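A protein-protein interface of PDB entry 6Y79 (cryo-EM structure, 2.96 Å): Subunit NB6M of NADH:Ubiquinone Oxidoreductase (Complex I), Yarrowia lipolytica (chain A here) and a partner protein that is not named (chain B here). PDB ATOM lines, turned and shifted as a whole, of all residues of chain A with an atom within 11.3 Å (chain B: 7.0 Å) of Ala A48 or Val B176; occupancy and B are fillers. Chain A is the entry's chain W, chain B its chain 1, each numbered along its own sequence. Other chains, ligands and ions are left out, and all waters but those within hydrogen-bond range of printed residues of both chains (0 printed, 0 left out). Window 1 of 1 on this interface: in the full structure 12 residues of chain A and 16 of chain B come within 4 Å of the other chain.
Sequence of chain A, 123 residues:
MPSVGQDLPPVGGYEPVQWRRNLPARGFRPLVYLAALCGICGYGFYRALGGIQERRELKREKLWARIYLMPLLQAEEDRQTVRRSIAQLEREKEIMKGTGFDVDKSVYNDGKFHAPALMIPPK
O of Pro B181 lies within hydrogen-bond range of SG of Cys A41 (3.2 Å). The backbone carbonyl oxygen (O) of Val B175 sits at hydrogen-bond distance from the guanidinium group (NH1) of Arg A47. The guanidinium group (NH2) of Arg A55 lies within hydrogen-bond range of the backbone carbonyl oxygen (O) of Phe B160, 2.8 Å away.
The backbone NH (N) of Ser B336 lies within hydrogen-bond range of the backbone carbonyl oxygen (O) of Leu B331 (3.2 Å).
Ile A40 touches Ile B180 (O to O, 3.5 Å). Ile B180 touches Cys A41 (O to CA, 3.8 Å). Gly A44 touches Pro B181. Phe A45 touches Pro B181 (N to CB, 3.7 Å). CZ of Phe A45 touches CD1 of Leu B182, at 3.7 Å. N of Ala A48 touches CG1 of Val B176, at 3.8 Å. Leu A49 touches Ser B336 (O to OG, 3.6 Å). Ile A52 touches Leu B331 (CD1 to CD2, 3.8 Å). Gln A53 touches Ser B336. CG2 of Thr B172 touches NH1 of Arg A55 (3.3 Å).
Of the printed residues of chain B, Gly A44 touches Pro B181 (3.4 Å). Printed residues of chain B within 4 Å of Ala A48: Val B176 (3.8 Å). Printed residues of chain A within 4 Å of Thr B172: Arg A55 (3.3 Å). No residue of chain A comes within 4 Å of Gln B173. Val B175 touches just one residue of chain A: Arg A47. Of chain A, only Arg A47 and Ala A48 come within 4 Å of Val B176. The nearest residue of chain B that does not touch Ala A48 is Pro B181 (4.4 Å). The nearest printed residue of chain B that does not touch Arg A47 is Arg B174 (5.5 Å).
Hydrophobic or aromatic side chains of chain A within 4 Å of the printed part of chain B: Ile A40, Phe A45, Ala A48, Leu A49 and Ile A52. Of the 18 printed residues of chain B, 9 touch a printed residue of chain A. Hydrophobic or aromatic side chains of chain B within 4 Å of the printed part of chain A: Val B176, Pro B181, Leu B182 and Leu B331. Among the printed residues, 15 pairs touch across the chains.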
ATOM      1  N   GLY A  39      -4.431  22.561 -22.614  1.00  0.00           N
ATOM      2  CA  GLY A  39      -4.558  22.835 -24.033  1.00  0.00           C
ATOM      3  C   GLY A  39      -3.582  23.892 -24.521  1.00  0.00           C
ATOM      4  O   GLY A  39      -2.940  23.724 -25.569  1.00  0.00           O
ATOM      5  N   ILE A  40      -3.426  24.975 -23.746  1.00  0.00           N
ATOM      6  CA  ILE A  40      -2.463  26.026 -24.076  1.00  0.00           C
ATOM      7  C   ILE A  40      -1.041  25.480 -24.044  1.00  0.00           C
ATOM      8  O   ILE A  40      -0.249  25.712 -24.968  1.00  0.00           O
ATOM      9  CB  ILE A  40      -2.625  27.216 -23.111  1.00  0.00           C
ATOM     10  CG1 ILE A  40      -3.961  27.936 -23.327  1.00  0.00           C
ATOM     11  CG2 ILE A  40      -1.475  28.201 -23.248  1.00  0.00           C
ATOM     12  CD1 ILE A  40      -4.218  28.371 -24.740  1.00  0.00           C
ATOM     13  N   CYS A  41      -0.706  24.721 -22.996  1.00  0.00           N
ATOM     14  CA  CYS A  41       0.646  24.192 -22.847  1.00  0.00           C
ATOM     15  C   CYS A  41       0.960  23.152 -23.915  1.00  0.00           C
ATOM     16  O   CYS A  41       2.073  23.120 -24.450  1.00  0.00           O
ATOM     17  CB  CYS A  41       0.832  23.604 -21.447  1.00  0.00           C
ATOM     18  SG  CYS A  41       0.857  24.812 -20.101  1.00  0.00           S
ATOM     19  N   GLY A  42      -0.017  22.309 -24.267  1.00  0.00           N
ATOM     20  CA  GLY A  42       0.214  21.318 -25.301  1.00  0.00           C
ATOM     21  C   GLY A  42       0.366  21.921 -26.679  1.00  0.00           C
ATOM     22  O   GLY A  42       1.179  21.449 -27.477  1.00  0.00           O
ATOM     23  N   TYR A  43      -0.382  22.988 -26.968  1.00  0.00           N
ATOM     24  CA  TYR A  43      -0.198  23.681 -28.237  1.00  0.00           C
ATOM     25  C   TYR A  43       1.157  24.378 -28.303  1.00  0.00           C
ATOM     26  O   TYR A  43       1.801  24.412 -29.365  1.00  0.00           O
ATOM     27  CB  TYR A  43      -1.319  24.687 -28.443  1.00  0.00           C
ATOM     28  CG  TYR A  43      -1.199  25.401 -29.745  1.00  0.00           C
ATOM     29  CD1 TYR A  43      -1.435  24.737 -30.936  1.00  0.00           C
ATOM     30  CD2 TYR A  43      -0.834  26.735 -29.792  1.00  0.00           C
ATOM     31  CE1 TYR A  43      -1.318  25.382 -32.138  1.00  0.00           C
ATOM     32  CE2 TYR A  43      -0.716  27.391 -30.986  1.00  0.00           C
ATOM     33  CZ  TYR A  43      -0.956  26.710 -32.155  1.00  0.00           C
ATOM     34  OH  TYR A  43      -0.837  27.366 -33.354  1.00  0.00           O
ATOM     35  N   GLY A  44       1.608  24.930 -27.176  1.00  0.00           N
ATOM     36  CA  GLY A  44       2.941  25.504 -27.136  1.00  0.00           C
ATOM     37  C   GLY A  44       4.031  24.469 -27.329  1.00  0.00           C
ATOM     38  O   GLY A  44       5.041  24.738 -27.978  1.00  0.00           O
ATOM     39  N   PHE A  45       3.840  23.270 -26.771  1.00  0.00           N
ATOM     40  CA  PHE A  45       4.806  22.192 -26.978  1.00  0.00           C
ATOM     41  C   PHE A  45       4.809  21.727 -28.424  1.00  0.00           C
ATOM     42  O   PHE A  45       5.862  21.355 -28.954  1.00  0.00           O
ATOM     43  CB  PHE A  45       4.505  21.018 -26.057  1.00  0.00           C
ATOM     44  CG  PHE A  45       5.248  21.062 -24.764  1.00  0.00           C
ATOM     45  CD1 PHE A  45       6.585  20.721 -24.707  1.00  0.00           C
ATOM     46  CD2 PHE A  45       4.603  21.432 -23.600  1.00  0.00           C
ATOM     47  CE1 PHE A  45       7.267  20.758 -23.509  1.00  0.00           C
ATOM     48  CE2 PHE A  45       5.277  21.475 -22.405  1.00  0.00           C
ATOM     49  CZ  PHE A  45       6.610  21.137 -22.359  1.00  0.00           C
ATOM     50  N   TYR A  46       3.634  21.731 -29.064  1.00  0.00           N
ATOM     51  CA  TYR A  46       3.525  21.448 -30.493  1.00  0.00           C
ATOM     52  C   TYR A  46       4.402  22.384 -31.311  1.00  0.00           C
ATOM     53  O   TYR A  46       5.255  21.933 -32.089  1.00  0.00           O
ATOM     54  CB  TYR A  46       2.062  21.558 -30.924  1.00  0.00           C
ATOM     55  CG  TYR A  46       1.819  21.487 -32.412  1.00  0.00           C
ATOM     56  CD1 TYR A  46       1.748  20.271 -33.053  1.00  0.00           C
ATOM     57  CD2 TYR A  46       1.623  22.636 -33.167  1.00  0.00           C
ATOM     58  CE1 TYR A  46       1.523  20.191 -34.410  1.00  0.00           C
ATOM     59  CE2 TYR A  46       1.400  22.567 -34.522  1.00  0.00           C
ATOM     60  CZ  TYR A  46       1.351  21.343 -35.137  1.00  0.00           C
ATOM     61  OH  TYR A  46       1.122  21.264 -36.488  1.00  0.00           O
ATOM     62  N   ARG A  47       4.233  23.692 -31.104  1.00  0.00           N
ATOM     63  CA  ARG A  47       5.011  24.667 -31.866  1.00  0.00           C
ATOM     64  C   ARG A  47       6.495  24.617 -31.526  1.00  0.00           C
ATOM     65  O   ARG A  47       7.342  24.738 -32.417  1.00  0.00           O
ATOM     66  CB  ARG A  47       4.471  26.066 -31.626  1.00  0.00           C
ATOM     67  CG  ARG A  47       3.104  26.278 -32.178  1.00  0.00           C
ATOM     68  CD  ARG A  47       2.715  27.711 -31.992  1.00  0.00           C
ATOM     69  NE  ARG A  47       3.600  28.597 -32.732  1.00  0.00           N
ATOM     70  CZ  ARG A  47       3.381  28.990 -33.979  1.00  0.00           C
ATOM     71  NH1 ARG A  47       4.237  29.795 -34.582  1.00  0.00           N
ATOM     72  NH2 ARG A  47       2.303  28.578 -34.624  1.00  0.00           N
ATOM     73  N   ALA A  48       6.829  24.408 -30.250  1.00  0.00           N
ATOM     74  CA  ALA A  48       8.225  24.400 -29.825  1.00  0.00           C
ATOM     75  C   ALA A  48       8.977  23.199 -30.381  1.00  0.00           C
ATOM     76  O   ALA A  48      10.093  23.341 -30.894  1.00  0.00           O
ATOM     77  CB  ALA A  48       8.303  24.415 -28.301  1.00  0.00           C
ATOM     78  N   LEU A  49       8.379  22.009 -30.296  1.00  0.00           N
ATOM     79  CA  LEU A  49       9.052  20.816 -30.786  1.00  0.00           C
ATOM     80  C   LEU A  49       9.108  20.799 -32.306  1.00  0.00           C
ATOM     81  O   LEU A  49      10.107  20.333 -32.879  1.00  0.00           O
ATOM     82  CB  LEU A  49       8.362  19.568 -30.239  1.00  0.00           C
ATOM     83  CG  LEU A  49       8.954  18.985 -28.949  1.00  0.00           C
ATOM     84  CD1 LEU A  49       8.804  19.908 -27.761  1.00  0.00           C
ATOM     85  CD2 LEU A  49       8.325  17.656 -28.628  1.00  0.00           C
ATOM     86  N   GLY A  50       8.084  21.355 -32.968  1.00  0.00           N
ATOM     87  CA  GLY A  50       8.176  21.566 -34.402  1.00  0.00           C
ATOM     88  C   GLY A  50       9.330  22.470 -34.788  1.00  0.00           C
ATOM     89  O   GLY A  50      10.119  22.128 -35.674  1.00  0.00           O
ATOM     90  N   GLY A  51       9.492  23.589 -34.074  1.00  0.00           N
ATOM     91  CA  GLY A  51      10.589  24.500 -34.354  1.00  0.00           C
ATOM     92  C   GLY A  51      11.965  23.926 -34.084  1.00  0.00           C
ATOM     93  O   GLY A  51      12.913  24.235 -34.813  1.00  0.00           O
ATOM     94  N   ILE A  52      12.093  23.071 -33.062  1.00  0.00           N
ATOM     95  CA  ILE A  52      13.371  22.403 -32.812  1.00  0.00           C
ATOM     96  C   ILE A  52      13.710  21.449 -33.952  1.00  0.00           C
ATOM     97  O   ILE A  52      14.867  21.378 -34.394  1.00  0.00           O
ATOM     98  CB  ILE A  52      13.358  21.666 -31.460  1.00  0.00           C
ATOM     99  CG1 ILE A  52      13.220  22.630 -30.297  1.00  0.00           C
ATOM    100  CG2 ILE A  52      14.642  20.904 -31.238  1.00  0.00           C
ATOM    101  CD1 ILE A  52      12.956  21.933 -28.995  1.00  0.00           C
ATOM    102  N   GLN A  53      12.711  20.725 -34.472  1.00  0.00           N
ATOM    103  CA  GLN A  53      12.990  19.817 -35.585  1.00  0.00           C
ATOM    104  C   GLN A  53      13.383  20.571 -36.857  1.00  0.00           C
ATOM    105  O   GLN A  53      14.295  20.137 -37.581  1.00  0.00           O
ATOM    106  CB  GLN A  53      11.796  18.904 -35.823  1.00  0.00           C
ATOM    107  CG  GLN A  53      11.573  17.947 -34.679  1.00  0.00           C
ATOM    108  CD  GLN A  53      10.313  17.149 -34.822  1.00  0.00           C
ATOM    109  OE1 GLN A  53       9.837  16.923 -35.926  1.00  0.00           O
ATOM    110  NE2 GLN A  53       9.752  16.724 -33.701  1.00  0.00           N
ATOM    111  N   GLU A  54      12.757  21.729 -37.109  1.00  0.00           N
ATOM    112  CA  GLU A  54      13.159  22.562 -38.248  1.00  0.00           C
ATOM    113  C   GLU A  54      14.567  23.076 -38.092  1.00  0.00           C
ATOM    114  O   GLU A  54      15.314  23.176 -39.067  1.00  0.00           O
ATOM    115  CB  GLU A  54      12.262  23.771 -38.380  1.00  0.00           C
ATOM    116  CG  GLU A  54      10.883  23.417 -38.558  1.00  0.00           C
ATOM    117  CD  GLU A  54      10.597  22.908 -39.889  1.00  0.00           C
ATOM    118  OE1 GLU A  54      11.213  23.372 -40.884  1.00  0.00           O
ATOM    119  OE2 GLU A  54       9.727  21.995 -40.013  1.00  0.00           O
ATOM    120  N   ARG A  55      14.900  23.512 -36.888  1.00  0.00           N
ATOM    121  CA  ARG A  55      16.220  24.054 -36.645  1.00  0.00           C
ATOM    122  C   ARG A  55      17.290  22.983 -36.800  1.00  0.00           C
ATOM    123  O   ARG A  55      18.391  23.270 -37.279  1.00  0.00           O
ATOM    124  CB  ARG A  55      16.233  24.670 -35.258  1.00  0.00           C
ATOM    125  CG  ARG A  55      17.413  25.482 -34.964  1.00  0.00           C
ATOM    126  CD  ARG A  55      17.169  26.244 -33.696  1.00  0.00           C
ATOM    127  NE  ARG A  55      17.156  25.395 -32.507  1.00  0.00           N
ATOM    128  CZ  ARG A  55      16.081  25.186 -31.758  1.00  0.00           C
ATOM    129  NH1 ARG A  55      14.927  25.745 -32.091  1.00  0.00           N
ATOM    130  NH2 ARG A  55      16.159  24.416 -30.685  1.00  0.00           N
ATOM    131  N   ARG A  56      16.951  21.737 -36.469  1.00  0.00           N
ATOM    132  CA  ARG A  56      17.845  20.617 -36.738  1.00  0.00           C
ATOM    133  C   ARG A  56      18.039  20.391 -38.237  1.00  0.00           C
ATOM    134  O   ARG A  56      19.166  20.147 -38.687  1.00  0.00           O
ATOM    135  CB  ARG A  56      17.297  19.364 -36.065  1.00  0.00           C
ATOM    136  CG  ARG A  56      18.098  18.116 -36.297  1.00  0.00           C
ATOM    137  CD  ARG A  56      17.371  16.941 -35.712  1.00  0.00           C
ATOM    138  NE  ARG A  56      16.155  16.638 -36.457  1.00  0.00           N
ATOM    139  CZ  ARG A  56      15.104  16.013 -35.941  1.00  0.00           C
ATOM    140  NH1 ARG A  56      15.116  15.637 -34.672  1.00  0.00           N
ATOM    141  NH2 ARG A  56      14.040  15.772 -36.691  1.00  0.00           N
ATOM    142  N   GLU A  57      16.966  20.487 -39.031  1.00  0.00           N
ATOM    143  CA  GLU A  57      17.122  20.328 -40.482  1.00  0.00           C
ATOM    144  C   GLU A  57      17.932  21.482 -41.090  1.00  0.00           C
ATOM    145  O   GLU A  57      18.737  21.280 -42.016  1.00  0.00           O
ATOM    146  CB  GLU A  57      15.748  20.218 -41.142  1.00  0.00           C
ATOM    147  CG  GLU A  57      14.876  19.080 -40.624  1.00  0.00           C
ATOM    148  CD  GLU A  57      15.337  17.692 -41.045  1.00  0.00           C
ATOM    149  OE1 GLU A  57      15.883  17.568 -42.158  1.00  0.00           O
ATOM    150  OE2 GLU A  57      15.132  16.715 -40.281  1.00  0.00           O
ATOM    151  N   PHE B 160      15.984  23.556 -24.331  1.00  0.00           N
ATOM    152  CA  PHE B 160      15.348  23.765 -25.623  1.00  0.00           C
ATOM    153  C   PHE B 160      16.255  24.409 -26.648  1.00  0.00           C
ATOM    154  O   PHE B 160      15.970  24.318 -27.843  1.00  0.00           O
ATOM    155  CB  PHE B 160      14.128  24.667 -25.477  1.00  0.00           C
ATOM    156  CG  PHE B 160      13.001  24.040 -24.754  1.00  0.00           C
ATOM    157  CD1 PHE B 160      12.853  22.671 -24.729  1.00  0.00           C
ATOM    158  CD2 PHE B 160      12.085  24.820 -24.094  1.00  0.00           C
ATOM    159  CE1 PHE B 160      11.811  22.098 -24.059  1.00  0.00           C
ATOM    160  CE2 PHE B 160      11.040  24.250 -23.425  1.00  0.00           C
ATOM    161  CZ  PHE B 160      10.905  22.886 -23.407  1.00  0.00           C
ATOM    162  N   ILE B 169      18.963  32.405 -27.936  1.00  0.00           N
ATOM    163  CA  ILE B 169      17.693  31.990 -27.338  1.00  0.00           C
ATOM    164  C   ILE B 169      16.542  32.814 -27.882  1.00  0.00           C
ATOM    165  O   ILE B 169      15.462  32.288 -28.172  1.00  0.00           O
ATOM    166  CB  ILE B 169      17.750  32.103 -25.809  1.00  0.00           C
ATOM    167  CG1 ILE B 169      18.852  31.229 -25.259  1.00  0.00           C
ATOM    168  CG2 ILE B 169      16.394  31.740 -25.177  1.00  0.00           C
ATOM    169  CD1 ILE B 169      18.804  31.178 -23.817  1.00  0.00           C
ATOM    170  N   ILE B 170      16.748  34.118 -28.025  1.00  0.00           N
ATOM    171  CA  ILE B 170      15.668  34.974 -28.488  1.00  0.00           C
ATOM    172  C   ILE B 170      15.376  34.722 -29.959  1.00  0.00           C
ATOM    173  O   ILE B 170      14.213  34.686 -30.366  1.00  0.00           O
ATOM    174  CB  ILE B 170      16.007  36.440 -28.190  1.00  0.00           C
ATOM    175  CG1 ILE B 170      16.336  36.566 -26.711  1.00  0.00           C
ATOM    176  CG2 ILE B 170      14.841  37.328 -28.522  1.00  0.00           C
ATOM    177  CD1 ILE B 170      16.649  37.936 -26.274  1.00  0.00           C
ATOM    178  N   THR B 172      15.781  31.838 -31.257  1.00  0.00           N
ATOM    179  CA  THR B 172      15.122  30.545 -31.172  1.00  0.00           C
ATOM    180  C   THR B 172      13.650  30.692 -30.796  1.00  0.00           C
ATOM    181  O   THR B 172      12.805  29.925 -31.267  1.00  0.00           O
ATOM    182  CB  THR B 172      15.895  29.690 -30.165  1.00  0.00           C
ATOM    183  OG1 THR B 172      17.253  29.581 -30.601  1.00  0.00           O
ATOM    184  CG2 THR B 172      15.347  28.327 -30.049  1.00  0.00           C
ATOM    185  N   GLN B 173      13.322  31.701 -29.996  1.00  0.00           N
ATOM    186  CA  GLN B 173      11.955  31.970 -29.558  1.00  0.00           C
ATOM    187  C   GLN B 173      11.103  32.673 -30.601  1.00  0.00           C
ATOM    188  O   GLN B 173      10.025  33.161 -30.255  1.00  0.00           O
ATOM    189  CB  GLN B 173      11.945  32.839 -28.305  1.00  0.00           C
ATOM    190  CG  GLN B 173      12.220  32.139 -27.009  1.00  0.00           C
ATOM    191  CD  GLN B 173      12.350  33.129 -25.893  1.00  0.00           C
ATOM    192  OE1 GLN B 173      11.924  34.262 -26.031  1.00  0.00           O
ATOM    193  NE2 GLN B 173      12.977  32.734 -24.806  1.00  0.00           N
ATOM    194  N   ARG B 174      11.561  32.779 -31.845  1.00  0.00           N
ATOM    195  CA  ARG B 174      10.755  33.421 -32.870  1.00  0.00           C
ATOM    196  C   ARG B 174       9.590  32.538 -33.282  1.00  0.00           C
ATOM    197  O   ARG B 174       8.535  33.046 -33.670  1.00  0.00           O
ATOM    198  CB  ARG B 174      11.636  33.769 -34.066  1.00  0.00           C
ATOM    199  CG  ARG B 174      10.960  34.590 -35.139  1.00  0.00           C
ATOM    200  CD  ARG B 174      11.934  34.960 -36.229  1.00  0.00           C
ATOM    201  NE  ARG B 174      12.991  35.827 -35.728  1.00  0.00           N
ATOM    202  CZ  ARG B 174      12.898  37.148 -35.677  1.00  0.00           C
ATOM    203  NH1 ARG B 174      11.798  37.755 -36.094  1.00  0.00           N
ATOM    204  NH2 ARG B 174      13.905  37.866 -35.210  1.00  0.00           N
ATOM    205  N   VAL B 175       9.746  31.221 -33.171  1.00  0.00           N
ATOM    206  CA  VAL B 175       8.680  30.325 -33.602  1.00  0.00           C
ATOM    207  C   VAL B 175       7.560  30.278 -32.561  1.00  0.00           C
ATOM    208  O   VAL B 175       6.377  30.213 -32.911  1.00  0.00           O
ATOM    209  CB  VAL B 175       9.264  28.937 -33.949  1.00  0.00           C
ATOM    210  CG1 VAL B 175       9.937  28.271 -32.770  1.00  0.00           C
ATOM    211  CG2 VAL B 175       8.205  28.048 -34.505  1.00  0.00           C
ATOM    212  N   VAL B 176       7.908  30.379 -31.278  1.00  0.00           N
ATOM    213  CA  VAL B 176       6.967  30.454 -30.164  1.00  0.00           C
ATOM    214  C   VAL B 176       7.758  30.985 -28.977  1.00  0.00           C
ATOM    215  O   VAL B 176       8.975  30.792 -28.902  1.00  0.00           O
ATOM    216  CB  VAL B 176       6.311  29.084 -29.870  1.00  0.00           C
ATOM    217  CG1 VAL B 176       7.302  28.083 -29.299  1.00  0.00           C
ATOM    218  CG2 VAL B 176       5.099  29.217 -28.966  1.00  0.00           C
ATOM    219  N   TRP B 177       7.106  31.685 -28.054  1.00  0.00           N
ATOM    220  CA  TRP B 177       7.787  32.042 -26.820  1.00  0.00           C
ATOM    221  C   TRP B 177       7.889  30.815 -25.922  1.00  0.00           C
ATOM    222  O   TRP B 177       7.377  29.747 -26.238  1.00  0.00           O
ATOM    223  CB  TRP B 177       7.059  33.170 -26.096  1.00  0.00           C
ATOM    224  CG  TRP B 177       7.062  34.465 -26.827  1.00  0.00           C
ATOM    225  CD1 TRP B 177       7.790  34.785 -27.927  1.00  0.00           C
ATOM    226  CD2 TRP B 177       6.281  35.616 -26.515  1.00  0.00           C
ATOM    227  NE1 TRP B 177       7.512  36.064 -28.323  1.00  0.00           N
ATOM    228  CE2 TRP B 177       6.585  36.597 -27.470  1.00  0.00           C
ATOM    229  CE3 TRP B 177       5.352  35.912 -25.518  1.00  0.00           C
ATOM    230  CZ2 TRP B 177       5.999  37.850 -27.456  1.00  0.00           C
ATOM    231  CZ3 TRP B 177       4.772  37.154 -25.508  1.00  0.00           C
ATOM    232  CH2 TRP B 177       5.088  38.103 -26.475  1.00  0.00           C
ATOM    233  N   TYR B 178       8.577  30.957 -24.797  1.00  0.00           N
ATOM    234  CA  TYR B 178       8.714  29.828 -23.889  1.00  0.00           C
ATOM    235  C   TYR B 178       7.748  29.885 -22.723  1.00  0.00           C
ATOM    236  O   TYR B 178       7.688  28.932 -21.944  1.00  0.00           O
ATOM    237  CB  TYR B 178      10.143  29.727 -23.358  1.00  0.00           C
ATOM    238  CG  TYR B 178      11.127  29.251 -24.389  1.00  0.00           C
ATOM    239  CD1 TYR B 178      10.710  28.512 -25.485  1.00  0.00           C
ATOM    240  CD2 TYR B 178      12.468  29.556 -24.280  1.00  0.00           C
ATOM    241  CE1 TYR B 178      11.598  28.092 -26.431  1.00  0.00           C
ATOM    242  CE2 TYR B 178      13.360  29.141 -25.224  1.00  0.00           C
ATOM    243  CZ  TYR B 178      12.916  28.409 -26.292  1.00  0.00           C
ATOM    244  OH  TYR B 178      13.800  27.984 -27.233  1.00  0.00           O
ATOM    245  N   CYS B 179       7.002  30.975 -22.577  1.00  0.00           N
ATOM    246  CA  CYS B 179       5.973  31.030 -21.548  1.00  0.00           C
ATOM    247  C   CYS B 179       4.717  30.289 -21.986  1.00  0.00           C
ATOM    248  O   CYS B 179       4.031  29.688 -21.159  1.00  0.00           O
ATOM    249  CB  CYS B 179       5.652  32.481 -21.214  1.00  0.00           C
ATOM    250  SG  CYS B 179       4.938  33.402 -22.582  1.00  0.00           S
ATOM    251  N   ILE B 180       4.405  30.321 -23.275  1.00  0.00           N
ATOM    252  CA  ILE B 180       3.214  29.674 -23.828  1.00  0.00           C
ATOM    253  C   ILE B 180       3.238  28.150 -23.665  1.00  0.00           C
ATOM    254  O   ILE B 180       2.207  27.592 -23.265  1.00  0.00           O
ATOM    255  CB  ILE B 180       3.001  30.119 -25.286  1.00  0.00           C
ATOM    256  CG1 ILE B 180       2.685  31.612 -25.314  1.00  0.00           C
ATOM    257  CG2 ILE B 180       1.873  29.362 -25.947  1.00  0.00           C
ATOM    258  CD1 ILE B 180       2.574  32.198 -26.694  1.00  0.00           C
ATOM    259  N   PRO B 181       4.354  27.405 -23.902  1.00  0.00           N
ATOM    260  CA  PRO B 181       4.342  26.004 -23.472  1.00  0.00           C
ATOM    261  C   PRO B 181       4.497  25.847 -21.972  1.00  0.00           C
ATOM    262  O   PRO B 181       3.799  25.053 -21.345  1.00  0.00           O
ATOM    263  CB  PRO B 181       5.544  25.391 -24.199  1.00  0.00           C
ATOM    264  CG  PRO B 181       5.969  26.358 -25.162  1.00  0.00           C
ATOM    265  CD  PRO B 181       5.598  27.672 -24.639  1.00  0.00           C
ATOM    266  N   LEU B 182       5.442  26.569 -21.392  1.00  0.00           N
ATOM    267  CA  LEU B 182       5.812  26.385 -19.991  1.00  0.00           C
ATOM    268  C   LEU B 182       5.240  27.501 -19.112  1.00  0.00           C
ATOM    269  O   LEU B 182       5.977  28.280 -18.519  1.00  0.00           O
ATOM    270  CB  LEU B 182       7.334  26.295 -19.871  1.00  0.00           C
ATOM    271  CG  LEU B 182       8.092  24.985 -20.169  1.00  0.00           C
ATOM    272  CD1 LEU B 182       7.957  24.470 -21.572  1.00  0.00           C
ATOM    273  CD2 LEU B 182       9.549  25.184 -19.921  1.00  0.00           C
ATOM    274  N   GLY B 248       9.221  36.620 -24.948  1.00  0.00           N
ATOM    275  CA  GLY B 248      10.055  36.984 -26.076  1.00  0.00           C
ATOM    276  C   GLY B 248      10.912  38.177 -25.713  1.00  0.00           C
ATOM    277  O   GLY B 248      10.446  39.128 -25.084  1.00  0.00           O
ATOM    278  N   LEU B 251      11.005  40.459 -29.298  1.00  0.00           N
ATOM    279  CA  LEU B 251      10.152  39.972 -30.365  1.00  0.00           C
ATOM    280  C   LEU B 251       8.709  40.370 -30.111  1.00  0.00           C
ATOM    281  O   LEU B 251       8.170  40.115 -29.030  1.00  0.00           O
ATOM    282  CB  LEU B 251      10.271  38.457 -30.480  1.00  0.00           C
ATOM    283  CG  LEU B 251      11.645  37.981 -30.914  1.00  0.00           C
ATOM    284  CD1 LEU B 251      11.613  36.504 -30.962  1.00  0.00           C
ATOM    285  CD2 LEU B 251      11.993  38.544 -32.270  1.00  0.00           C
ATOM    286  N   LEU B 331      11.055  15.834 -24.977  1.00  0.00           N
ATOM    287  CA  LEU B 331      12.045  16.046 -26.029  1.00  0.00           C
ATOM    288  C   LEU B 331      12.606  14.737 -26.560  1.00  0.00           C
ATOM    289  O   LEU B 331      13.227  14.728 -27.624  1.00  0.00           O
ATOM    290  CB  LEU B 331      13.200  16.897 -25.539  1.00  0.00           C
ATOM    291  CG  LEU B 331      13.050  18.392 -25.261  1.00  0.00           C
ATOM    292  CD1 LEU B 331      14.377  18.926 -24.803  1.00  0.00           C
ATOM    293  CD2 LEU B 331      12.596  19.110 -26.490  1.00  0.00           C
ATOM    294  N   SER B 336      13.318  15.116 -30.787  1.00  0.00           N
ATOM    295  CA  SER B 336      13.472  16.554 -30.882  1.00  0.00           C
ATOM    296  C   SER B 336      14.531  16.937 -29.849  1.00  0.00           C
ATOM    297  O   SER B 336      14.223  17.325 -28.723  1.00  0.00           O
ATOM    298  CB  SER B 336      12.149  17.256 -30.627  1.00  0.00           C
ATOM    299  OG  SER B 336      12.281  18.662 -30.612  1.00  0.00           O
